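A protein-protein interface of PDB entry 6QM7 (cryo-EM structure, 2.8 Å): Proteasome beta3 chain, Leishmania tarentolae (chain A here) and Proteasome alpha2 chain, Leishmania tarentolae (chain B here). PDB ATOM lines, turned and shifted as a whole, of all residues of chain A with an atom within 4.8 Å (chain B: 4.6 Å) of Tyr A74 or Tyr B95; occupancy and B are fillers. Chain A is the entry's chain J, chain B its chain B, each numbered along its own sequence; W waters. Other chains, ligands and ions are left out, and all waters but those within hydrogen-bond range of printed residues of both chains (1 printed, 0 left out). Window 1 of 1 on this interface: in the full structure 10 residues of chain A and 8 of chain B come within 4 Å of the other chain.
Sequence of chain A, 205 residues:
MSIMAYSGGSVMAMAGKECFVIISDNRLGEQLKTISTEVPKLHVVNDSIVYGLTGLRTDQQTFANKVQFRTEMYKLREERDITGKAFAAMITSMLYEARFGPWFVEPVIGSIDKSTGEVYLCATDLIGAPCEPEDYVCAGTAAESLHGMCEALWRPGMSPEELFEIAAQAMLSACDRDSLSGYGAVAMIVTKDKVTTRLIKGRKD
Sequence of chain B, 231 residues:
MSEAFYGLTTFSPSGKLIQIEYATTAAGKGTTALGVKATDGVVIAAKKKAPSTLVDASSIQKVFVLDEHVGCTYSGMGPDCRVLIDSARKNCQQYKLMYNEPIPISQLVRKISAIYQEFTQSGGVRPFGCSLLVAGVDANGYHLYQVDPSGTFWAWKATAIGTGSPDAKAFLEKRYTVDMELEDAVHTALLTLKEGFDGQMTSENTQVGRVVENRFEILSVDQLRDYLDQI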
ATOM      1  N   ARG A  70      19.659   3.049  15.874  1.00  0.00           N
ATOM      2  CA  ARG A  70      19.186   1.912  15.055  1.00  0.00           C
ATOM      3  C   ARG A  70      19.228   0.620  15.876  1.00  0.00           C
ATOM      4  O   ARG A  70      18.258  -0.144  15.782  1.00  0.00           O
ATOM      5  CB  ARG A  70      20.022   1.806  13.782  1.00  0.00           C
ATOM      6  CG  ARG A  70      19.829   2.963  12.809  1.00  0.00           C
ATOM      7  CD  ARG A  70      18.482   2.930  12.144  1.00  0.00           C
ATOM      8  NE  ARG A  70      18.346   1.650  11.472  1.00  0.00           N
ATOM      9  CZ  ARG A  70      18.851   1.355  10.276  1.00  0.00           C
ATOM     10  NH1 ARG A  70      19.519   2.263   9.575  1.00  0.00           N
ATOM     11  NH2 ARG A  70      18.668   0.140   9.782  1.00  0.00           N
ATOM     12  N   THR A  71      20.286   0.390  16.655  1.00  0.00           N
ATOM     13  CA  THR A  71      20.466  -0.843  17.459  1.00  0.00           C
ATOM     14  C   THR A  71      19.535  -0.850  18.661  1.00  0.00           C
ATOM     15  O   THR A  71      19.165  -1.965  19.065  1.00  0.00           O
ATOM     16  CB  THR A  71      21.873  -1.025  18.020  1.00  0.00           C
ATOM     17  OG1 THR A  71      22.143   0.079  18.882  1.00  0.00           O
ATOM     18  CG2 THR A  71      22.923  -1.151  16.940  1.00  0.00           C
ATOM     19  N   GLU A  72      19.206   0.307  19.238  1.00  0.00           N
ATOM     20  CA  GLU A  72      18.233   0.383  20.363  1.00  0.00           C
ATOM     21  C   GLU A  72      16.805   0.217  19.836  1.00  0.00           C
ATOM     22  O   GLU A  72      16.011  -0.401  20.553  1.00  0.00           O
ATOM     23  CB  GLU A  72      18.364   1.687  21.152  1.00  0.00           C
ATOM     24  CG  GLU A  72      19.556   1.716  22.101  1.00  0.00           C
ATOM     25  CD  GLU A  72      19.605   0.633  23.179  1.00  0.00           C
ATOM     26  OE1 GLU A  72      20.719   0.388  23.715  1.00  0.00           O
ATOM     27  OE2 GLU A  72      18.538   0.031  23.488  1.00  0.00           O
ATOM     28  N   MET A  73      16.484   0.778  18.666  1.00  0.00           N
ATOM     29  CA  MET A  73      15.149   0.633  18.023  1.00  0.00           C
ATOM     30  C   MET A  73      14.927  -0.841  17.711  1.00  0.00           C
ATOM     31  O   MET A  73      13.818  -1.328  17.924  1.00  0.00           O
ATOM     32  CB  MET A  73      15.012   1.408  16.705  1.00  0.00           C
ATOM     33  CG  MET A  73      13.994   2.551  16.709  1.00  0.00           C
ATOM     34  SD  MET A  73      12.632   2.401  17.901  1.00  0.00           S
ATOM     35  CE  MET A  73      11.250   2.006  16.830  1.00  0.00           C
ATOM     36  N   TYR A  74      15.947  -1.487  17.156  1.00  0.00           N
ATOM     37  CA  TYR A  74      15.954  -2.923  16.798  1.00  0.00           C
ATOM     38  C   TYR A  74      15.578  -3.719  18.039  1.00  0.00           C
ATOM     39  O   TYR A  74      14.662  -4.514  17.986  1.00  0.00           O
ATOM     40  CB  TYR A  74      17.341  -3.324  16.303  1.00  0.00           C
ATOM     41  CG  TYR A  74      17.447  -4.707  15.729  1.00  0.00           C
ATOM     42  CD1 TYR A  74      17.435  -4.901  14.359  1.00  0.00           C
ATOM     43  CD2 TYR A  74      17.600  -5.816  16.541  1.00  0.00           C
ATOM     44  CE1 TYR A  74      17.560  -6.165  13.808  1.00  0.00           C
ATOM     45  CE2 TYR A  74      17.717  -7.088  16.007  1.00  0.00           C
ATOM     46  CZ  TYR A  74      17.698  -7.269  14.632  1.00  0.00           C
ATOM     47  OH  TYR A  74      17.824  -8.513  14.069  1.00  0.00           O
ATOM     48  N   LYS A  75      16.279  -3.447  19.132  1.00  0.00           N
ATOM     49  CA  LYS A  75      16.175  -4.160  20.424  1.00  0.00           C
ATOM     50  C   LYS A  75      14.734  -4.060  20.942  1.00  0.00           C
ATOM     51  O   LYS A  75      14.277  -5.017  21.610  1.00  0.00           O
ATOM     52  CB  LYS A  75      17.193  -3.560  21.402  1.00  0.00           C
ATOM     53  CG  LYS A  75      18.004  -4.543  22.234  1.00  0.00           C
ATOM     54  CD  LYS A  75      17.398  -4.856  23.595  1.00  0.00           C
ATOM     55  CE  LYS A  75      18.362  -5.559  24.533  1.00  0.00           C
ATOM     56  NZ  LYS A  75      18.551  -6.987  24.169  1.00  0.00           N
ATOM     57  N   LEU A  76      14.056  -2.942  20.686  1.00  0.00           N
ATOM     58  CA  LEU A  76      12.663  -2.716  21.142  1.00  0.00           C
ATOM     59  C   LEU A  76      11.703  -3.451  20.216  1.00  0.00           C
ATOM     60  O   LEU A  76      10.900  -4.257  20.719  1.00  0.00           O
ATOM     61  CB  LEU A  76      12.341  -1.225  21.140  1.00  0.00           C
ATOM     62  CG  LEU A  76      13.015  -0.415  22.237  1.00  0.00           C
ATOM     63  CD1 LEU A  76      12.973   1.073  21.918  1.00  0.00           C
ATOM     64  CD2 LEU A  76      12.363  -0.689  23.582  1.00  0.00           C
ATOM     65  N   ARG A  77      11.765  -3.142  18.923  1.00  0.00           N
ATOM     66  CA  ARG A  77      10.909  -3.759  17.885  1.00  0.00           C
ATOM     67  C   ARG A  77      11.110  -5.277  17.926  1.00  0.00           C
ATOM     68  O   ARG A  77      10.152  -5.991  18.252  1.00  0.00           O
ATOM     69  CB  ARG A  77      11.221  -3.164  16.511  1.00  0.00           C
ATOM     70  CG  ARG A  77      10.560  -1.820  16.227  1.00  0.00           C
ATOM     71  CD  ARG A  77      10.448  -1.547  14.730  1.00  0.00           C
ATOM     72  NE  ARG A  77      11.769  -1.749  14.139  1.00  0.00           N
ATOM     73  CZ  ARG A  77      12.683  -0.802  13.875  1.00  0.00           C
ATOM     74  NH1 ARG A  77      13.861  -1.162  13.380  1.00  0.00           N
ATOM     75  NH2 ARG A  77      12.429   0.485  14.087  1.00  0.00           N
ATOM     76  N   GLU A  78      12.330  -5.739  17.672  1.00  0.00           N
ATOM     77  CA  GLU A  78      12.670  -7.170  17.446  1.00  0.00           C
ATOM     78  C   GLU A  78      12.633  -7.973  18.741  1.00  0.00           C
ATOM     79  O   GLU A  78      12.534  -9.210  18.633  1.00  0.00           O
ATOM     80  CB  GLU A  78      14.074  -7.327  16.872  1.00  0.00           C
ATOM     81  CG  GLU A  78      14.274  -6.532  15.595  1.00  0.00           C
ATOM     82  CD  GLU A  78      14.340  -7.310  14.297  1.00  0.00           C
ATOM     83  OE1 GLU A  78      14.126  -6.671  13.252  1.00  0.00           O
ATOM     84  OE2 GLU A  78      14.631  -8.528  14.334  1.00  0.00           O
ATOM     85  N   GLU A  79      12.751  -7.318  19.897  1.00  0.00           N
ATOM     86  CA  GLU A  79      12.718  -7.979  21.224  1.00  0.00           C
ATOM     87  C   GLU A  79      13.878  -8.980  21.309  1.00  0.00           C
ATOM     88  O   GLU A  79      13.689 -10.067  21.861  1.00  0.00           O
ATOM     89  CB  GLU A  79      11.343  -8.621  21.438  1.00  0.00           C
ATOM     90  CG  GLU A  79      10.443  -7.825  22.357  1.00  0.00           C
ATOM     91  CD  GLU A  79       8.954  -7.849  22.037  1.00  0.00           C
ATOM     92  OE1 GLU A  79       8.535  -7.075  21.137  1.00  0.00           O
ATOM     93  OE2 GLU A  79       8.213  -8.645  22.680  1.00  0.00           O
ATOM     94  N   ARG A  80      15.040  -8.624  20.757  1.00  0.00           N
ATOM     95  CA  ARG A  80      16.282  -9.435  20.838  1.00  0.00           C
ATOM     96  C   ARG A  80      17.477  -8.551  20.515  1.00  0.00           C
ATOM     97  O   ARG A  80      17.277  -7.480  19.943  1.00  0.00           O
ATOM     98  CB  ARG A  80      16.280 -10.627  19.874  1.00  0.00           C
ATOM     99  CG  ARG A  80      15.991 -10.261  18.428  1.00  0.00           C
ATOM    100  CD  ARG A  80      16.364 -11.357  17.454  1.00  0.00           C
ATOM    101  NE  ARG A  80      16.169 -10.931  16.073  1.00  0.00           N
ATOM    102  CZ  ARG A  80      16.525 -11.633  14.999  1.00  0.00           C
ATOM    103  NH1 ARG A  80      17.101 -12.817  15.131  1.00  0.00           N
ATOM    104  NH2 ARG A  80      16.299 -11.150  13.787  1.00  0.00           N
ATOM    105  N   ASP A  81      18.665  -9.006  20.905  1.00  0.00           N
ATOM    106  CA  ASP A  81      19.941  -8.345  20.564  1.00  0.00           C
ATOM    107  C   ASP A  81      20.139  -8.570  19.079  1.00  0.00           C
ATOM    108  O   ASP A  81      19.867  -9.690  18.611  1.00  0.00           O
ATOM    109  CB  ASP A  81      21.109  -8.909  21.376  1.00  0.00           C
ATOM    110  CG  ASP A  81      21.208  -8.384  22.805  1.00  0.00           C
ATOM    111  OD1 ASP A  81      21.526  -9.197  23.709  1.00  0.00           O
ATOM    112  OD2 ASP A  81      20.993  -7.161  23.007  1.00  0.00           O
ATOM    113  N   ILE A  82      20.579  -7.541  18.372  1.00  0.00           N
ATOM    114  CA  ILE A  82      21.041  -7.680  16.965  1.00  0.00           C
ATOM    115  C   ILE A  82      22.293  -8.573  16.969  1.00  0.00           C
ATOM    116  O   ILE A  82      23.042  -8.554  17.969  1.00  0.00           O
ATOM    117  CB  ILE A  82      21.225  -6.293  16.317  1.00  0.00           C
ATOM    118  CG1 ILE A  82      21.312  -6.379  14.792  1.00  0.00           C
ATOM    119  CG2 ILE A  82      22.408  -5.541  16.899  1.00  0.00           C
ATOM    120  CD1 ILE A  82      21.133  -5.046  14.096  1.00  0.00           C
ATOM    121  N   ALA A  86      23.806  -9.225  11.000  1.00  0.00           N
ATOM    122  CA  ALA A  86      22.702  -8.255  10.816  1.00  0.00           C
ATOM    123  C   ALA A  86      23.202  -6.842  11.101  1.00  0.00           C
ATOM    124  O   ALA A  86      22.894  -5.929  10.323  1.00  0.00           O
ATOM    125  CB  ALA A  86      21.546  -8.615  11.719  1.00  0.00           C
ATOM    126  N   ASN B  91       8.158  -6.080   2.457  1.00  0.00           N
ATOM    127  CA  ASN B  91       8.747  -5.960   3.818  1.00  0.00           C
ATOM    128  C   ASN B  91       9.779  -7.064   4.061  1.00  0.00           C
ATOM    129  O   ASN B  91      10.806  -6.760   4.661  1.00  0.00           O
ATOM    130  CB  ASN B  91       7.668  -5.979   4.900  1.00  0.00           C
ATOM    131  CG  ASN B  91       6.894  -4.686   4.920  1.00  0.00           C
ATOM    132  OD1 ASN B  91       7.438  -3.637   4.577  1.00  0.00           O
ATOM    133  ND2 ASN B  91       5.629  -4.758   5.306  1.00  0.00           N
ATOM    134  N   CYS B  92       9.507  -8.296   3.643  1.00  0.00           N
ATOM    135  CA  CYS B  92      10.440  -9.429   3.827  1.00  0.00           C
ATOM    136  C   CYS B  92      11.749  -9.131   3.095  1.00  0.00           C
ATOM    137  O   CYS B  92      12.824  -9.457   3.643  1.00  0.00           O
ATOM    138  CB  CYS B  92       9.838 -10.733   3.332  1.00  0.00           C
ATOM    139  SG  CYS B  92       8.405 -11.243   4.309  1.00  0.00           S
ATOM    140  N   GLN B  93      11.635  -8.555   1.899  1.00  0.00           N
ATOM    141  CA  GLN B  93      12.777  -8.250   1.010  1.00  0.00           C
ATOM    142  C   GLN B  93      13.501  -7.014   1.542  1.00  0.00           C
ATOM    143  O   GLN B  93      14.734  -7.046   1.550  1.00  0.00           O
ATOM    144  CB  GLN B  93      12.315  -8.082  -0.438  1.00  0.00           C
ATOM    145  CG  GLN B  93      12.094  -9.404  -1.168  1.00  0.00           C
ATOM    146  CD  GLN B  93      13.210 -10.411  -0.984  1.00  0.00           C
ATOM    147  OE1 GLN B  93      14.385 -10.132  -1.234  1.00  0.00           O
ATOM    148  NE2 GLN B  93      12.843 -11.601  -0.531  1.00  0.00           N
ATOM    149  N   GLN B  94      12.777  -5.978   1.965  1.00  0.00           N
ATOM    150  CA  GLN B  94      13.375  -4.747   2.547  1.00  0.00           C
ATOM    151  C   GLN B  94      14.220  -5.118   3.760  1.00  0.00           C
ATOM    152  O   GLN B  94      15.323  -4.573   3.913  1.00  0.00           O
ATOM    153  CB  GLN B  94      12.307  -3.749   2.992  1.00  0.00           C
ATOM    154  CG  GLN B  94      11.886  -2.788   1.894  1.00  0.00           C
ATOM    155  CD  GLN B  94      10.784  -1.888   2.396  1.00  0.00           C
ATOM    156  OE1 GLN B  94      10.930  -1.229   3.429  1.00  0.00           O
ATOM    157  NE2 GLN B  94       9.660  -1.875   1.686  1.00  0.00           N
ATOM    158  N   TYR B  95      13.689  -6.001   4.589  1.00  0.00           N
ATOM    159  CA  TYR B  95      14.351  -6.514   5.805  1.00  0.00           C
ATOM    160  C   TYR B  95      15.621  -7.269   5.406  1.00  0.00           C
ATOM    161  O   TYR B  95      16.636  -7.046   6.068  1.00  0.00           O
ATOM    162  CB  TYR B  95      13.376  -7.369   6.616  1.00  0.00           C
ATOM    163  CG  TYR B  95      13.867  -7.678   8.001  1.00  0.00           C
ATOM    164  CD1 TYR B  95      13.424  -6.977   9.104  1.00  0.00           C
ATOM    165  CD2 TYR B  95      14.831  -8.638   8.193  1.00  0.00           C
ATOM    166  CE1 TYR B  95      13.907  -7.252  10.371  1.00  0.00           C
ATOM    167  CE2 TYR B  95      15.331  -8.921   9.448  1.00  0.00           C
ATOM    168  CZ  TYR B  95      14.876  -8.225  10.547  1.00  0.00           C
ATOM    169  OH  TYR B  95      15.422  -8.555  11.756  1.00  0.00           O
ATOM    170  N   LYS B  96      15.574  -8.132   4.389  1.00  0.00           N
ATOM    171  CA  LYS B  96      16.757  -8.909   3.918  1.00  0.00           C
ATOM    172  C   LYS B  96      17.841  -7.957   3.424  1.00  0.00           C
ATOM    173  O   LYS B  96      18.997  -8.149   3.785  1.00  0.00           O
ATOM    174  CB  LYS B  96      16.427  -9.865   2.774  1.00  0.00           C
ATOM    175  CG  LYS B  96      15.870 -11.209   3.213  1.00  0.00           C
ATOM    176  CD  LYS B  96      16.600 -12.385   2.600  1.00  0.00           C
ATOM    177  CE  LYS B  96      15.921 -13.713   2.886  1.00  0.00           C
ATOM    178  NZ  LYS B  96      14.912 -14.061   1.854  1.00  0.00           N
ATOM    179  N   LEU B  97      17.464  -6.981   2.609  1.00  0.00           N
ATOM    180  CA  LEU B  97      18.386  -5.946   2.086  1.00  0.00           C
ATOM    181  C   LEU B  97      19.083  -5.233   3.240  1.00  0.00           C
ATOM    182  O   LEU B  97      20.303  -5.026   3.138  1.00  0.00           O
ATOM    183  CB  LEU B  97      17.597  -4.957   1.233  1.00  0.00           C
ATOM    184  CG  LEU B  97      17.248  -5.494  -0.146  1.00  0.00           C
ATOM    185  CD1 LEU B  97      16.199  -4.626  -0.828  1.00  0.00           C
ATOM    186  CD2 LEU B  97      18.512  -5.600  -0.986  1.00  0.00           C
ATOM    187  N   MET B  98      18.348  -4.872   4.292  1.00  0.00           N
ATOM    188  CA  MET B  98      18.952  -4.155   5.440  1.00  0.00           C
ATOM    189  C   MET B  98      19.815  -5.126   6.231  1.00  0.00           C
ATOM    190  O   MET B  98      21.023  -4.892   6.275  1.00  0.00           O
ATOM    191  CB  MET B  98      17.922  -3.535   6.375  1.00  0.00           C
ATOM    192  CG  MET B  98      18.525  -2.485   7.270  1.00  0.00           C
ATOM    193  SD  MET B  98      17.629  -0.929   7.091  1.00  0.00           S
ATOM    194  CE  MET B  98      15.983  -1.439   7.594  1.00  0.00           C
ATOM    195  N   TYR B  99      19.236  -6.193   6.779  1.00  0.00           N
ATOM    196  CA  TYR B  99      19.878  -7.003   7.844  1.00  0.00           C
ATOM    197  C   TYR B  99      20.470  -8.303   7.307  1.00  0.00           C
ATOM    198  O   TYR B  99      21.086  -8.994   8.102  1.00  0.00           O
ATOM    199  CB  TYR B  99      18.876  -7.276   8.960  1.00  0.00           C
ATOM    200  CG  TYR B  99      18.343  -6.023   9.599  1.00  0.00           C
ATOM    201  CD1 TYR B  99      19.178  -5.186  10.316  1.00  0.00           C
ATOM    202  CD2 TYR B  99      17.009  -5.669   9.486  1.00  0.00           C
ATOM    203  CE1 TYR B  99      18.707  -4.030  10.914  1.00  0.00           C
ATOM    204  CE2 TYR B  99      16.518  -4.517  10.082  1.00  0.00           C
ATOM    205  CZ  TYR B  99      17.371  -3.692  10.796  1.00  0.00           C
ATOM    206  OH  TYR B  99      16.904  -2.550  11.377  1.00  0.00           O
ATOM    207  N   ASN B 100      20.304  -8.629   6.028  1.00  0.00           N
ATOM    208  CA  ASN B 100      20.937  -9.821   5.397  1.00  0.00           C
ATOM    209  C   ASN B 100      20.559 -11.041   6.237  1.00  0.00           C
ATOM    210  O   ASN B 100      21.432 -11.803   6.632  1.00  0.00           O
ATOM    211  CB  ASN B 100      22.435  -9.575   5.187  1.00  0.00           C
ATOM    212  CG  ASN B 100      23.127 -10.671   4.410  1.00  0.00           C
ATOM    213  OD1 ASN B 100      24.324 -10.885   4.580  1.00  0.00           O
ATOM    214  ND2 ASN B 100      22.388 -11.386   3.574  1.00  0.00           N
ATOM    215  N   GLU B 101      19.267 -11.180   6.488  1.00  0.00           N
ATOM    216  CA  GLU B 101      18.656 -12.069   7.503  1.00  0.00           C
ATOM    217  C   GLU B 101      17.174 -12.189   7.181  1.00  0.00           C
ATOM    218  O   GLU B 101      16.558 -11.184   6.837  1.00  0.00           O
ATOM    219  CB  GLU B 101      18.749 -11.457   8.906  1.00  0.00           C
ATOM    220  CG  GLU B 101      19.800 -12.073   9.814  1.00  0.00           C
ATOM    221  CD  GLU B 101      19.390 -12.179  11.279  1.00  0.00           C
ATOM    222  OE1 GLU B 101      20.227 -11.844  12.162  1.00  0.00           O
ATOM    223  OE2 GLU B 101      18.245 -12.629  11.545  1.00  0.00           O
ATOM    224  N   PRO B 102      16.538 -13.369   7.318  1.00  0.00           N
ATOM    225  CA  PRO B 102      15.091 -13.472   7.141  1.00  0.00           C
ATOM    226  C   PRO B 102      14.352 -12.628   8.187  1.00  0.00           C
ATOM    227  O   PRO B 102      14.781 -12.600   9.326  1.00  0.00           O
ATOM    228  CB  PRO B 102      14.785 -14.959   7.327  1.00  0.00           C
ATOM    229  CG  PRO B 102      16.116 -15.633   7.104  1.00  0.00           C
ATOM    230  CD  PRO B 102      17.152 -14.661   7.625  1.00  0.00           C
ATOM    231  N   ILE B 103      13.289 -11.936   7.776  1.00  0.00           N
ATOM    232  CA  ILE B 103      12.456 -11.141   8.722  1.00  0.00           C
ATOM    233  C   ILE B 103      11.861 -12.116   9.733  1.00  0.00           C
ATOM    234  O   ILE B 103      11.367 -13.177   9.367  1.00  0.00           O
ATOM    235  CB  ILE B 103      11.398 -10.284   8.003  1.00  0.00           C
ATOM    236  CG1 ILE B 103      10.752  -9.304   8.975  1.00  0.00           C
ATOM    237  CG2 ILE B 103      10.346 -11.120   7.282  1.00  0.00           C
ATOM    238  CD1 ILE B 103       9.972  -8.215   8.304  1.00  0.00           C
ATOM    239  N   PRO B 104      11.983 -11.846  11.044  1.00  0.00           N
ATOM    240  CA  PRO B 104      11.255 -12.613  12.043  1.00  0.00           C
ATOM    241  C   PRO B 104       9.752 -12.491  11.815  1.00  0.00           C
ATOM    242  O   PRO B 104       9.339 -11.512  11.280  1.00  0.00           O
ATOM    243  CB  PRO B 104      11.633 -11.938  13.364  1.00  0.00           C
ATOM    244  CG  PRO B 104      12.970 -11.305  13.082  1.00  0.00           C
ATOM    245  CD  PRO B 104      12.862 -10.840  11.648  1.00  0.00           C
ATOM    246  N   LYS B 111       4.361  -5.436  10.921  1.00  0.00           N
ATOM    247  CA  LYS B 111       4.390  -4.560   9.717  1.00  0.00           C
ATOM    248  C   LYS B 111       3.079  -4.690   8.934  1.00  0.00           C
ATOM    249  O   LYS B 111       2.657  -3.684   8.343  1.00  0.00           O
ATOM    250  CB  LYS B 111       5.594  -4.867   8.820  1.00  0.00           C
ATOM    251  CG  LYS B 111       6.856  -4.131   9.232  1.00  0.00           C
ATOM    252  CD  LYS B 111       8.120  -4.612   8.580  1.00  0.00           C
ATOM    253  CE  LYS B 111       9.309  -3.820   9.084  1.00  0.00           C
ATOM    254  NZ  LYS B 111      10.564  -4.201   8.394  1.00  0.00           N
HETATM  255  O   HOH W   1      17.524  -0.544  13.029  1.00  0.00           O
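SD of Met B98 is in hydrogen-bond range of NH2 of Arg A70 (3.1 Å).
The side-chain hydroxyl (OH) of Tyr B95 is in hydrogen-bond range of the side-chain hydroxyl (OH) of Tyr A74, 3.3 Å away.
The side-chain carboxylate (OE2) of Glu A78 sits at hydrogen-bond distance from the side-chain hydroxyl (OH) of Tyr B95 (2.7 Å).
NH2 of Arg A80 sits at hydrogen-bond distance from OH of Tyr B95 (3.4 Å).
The guanidinium group (NH2) of Arg A80 is in salt-bridge range of the side-chain carboxylate (OE2) of Glu B101.
OE2 of Glu A78 is in hydrogen-bond range of OH of Tyr A74 (3.2 Å).
OH of Tyr A74 is in hydrogen-bond range of NH2 of Arg A80 (3.1 Å).
OE2 of Glu A78 lies within salt-bridge range of NH2 of Arg A80.
Among the printed residues, pairs that only touch across the chains: Ala A86 with Tyr B99 (3.2 Å), Arg A80 with Pro B104 (3.4 Å), Glu A78 with Pro B104 (3.5 Å), Ala A86 with Glu B101 (3.5 Å), Arg A70 with Tyr B99 (3.6 Å), Tyr A74 with Tyr B99 (3.8 Å) and Arg A77 with Tyr B99 (3.9 Å).
Of chain B, only Tyr B95 and Tyr B99 come within 4 Å of Tyr A74.
Of the printed residues of chain B, Arg A70 touches Met B98 (3.1 Å) and Tyr B99 (3.6 Å).
Printed residues of chain B within 4 Å of Arg A80: Tyr B95 (3.4 Å), Glu B101 (3.3 Å) and Pro B104 (3.4 Å).
Printed residues of chain A within 4 Å of Tyr B99: Arg A70, Tyr A74, Arg A77 and Ala A86.
Of the printed residues of chain A, Pro B104 touches Glu A78 (3.5 Å) and Arg A80 (3.4 Å).
Of the printed residues of chain B, Glu A78 touches Tyr B95 (2.7 Å) and Pro B104 (3.5 Å).
Leu A76 touches none of the printed residues of chain B.
Glu A79 touches none of the printed residues of chain B.
The nearest residue of chain B that does not touch Tyr A74 is Glu B101 (4.5 Å).
The nearest printed residue of chain A that does not touch Glu B101 is Tyr A74 (4.5 Å).
Along chain B the printed residues that touch a printed residue of chain A span positions 95 to 104.
Of the 14 printed residues of chain A, 6 touch a printed residue of chain B.
Along chain A the printed residues that touch a printed residue of chain B span positions 70 to 86.
Among the printed residues, Asp or Glu carboxylates within 4 Å of a Lys or Arg side-chain nitrogen of the other chain: Arg A80 with Glu B101.
Water W1 lies within hydrogen-bond range of the side-chain hydroxyl of Tyr B99 (2.7 Å) and the guanidinium group of Arg A70 (2.8 Å).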
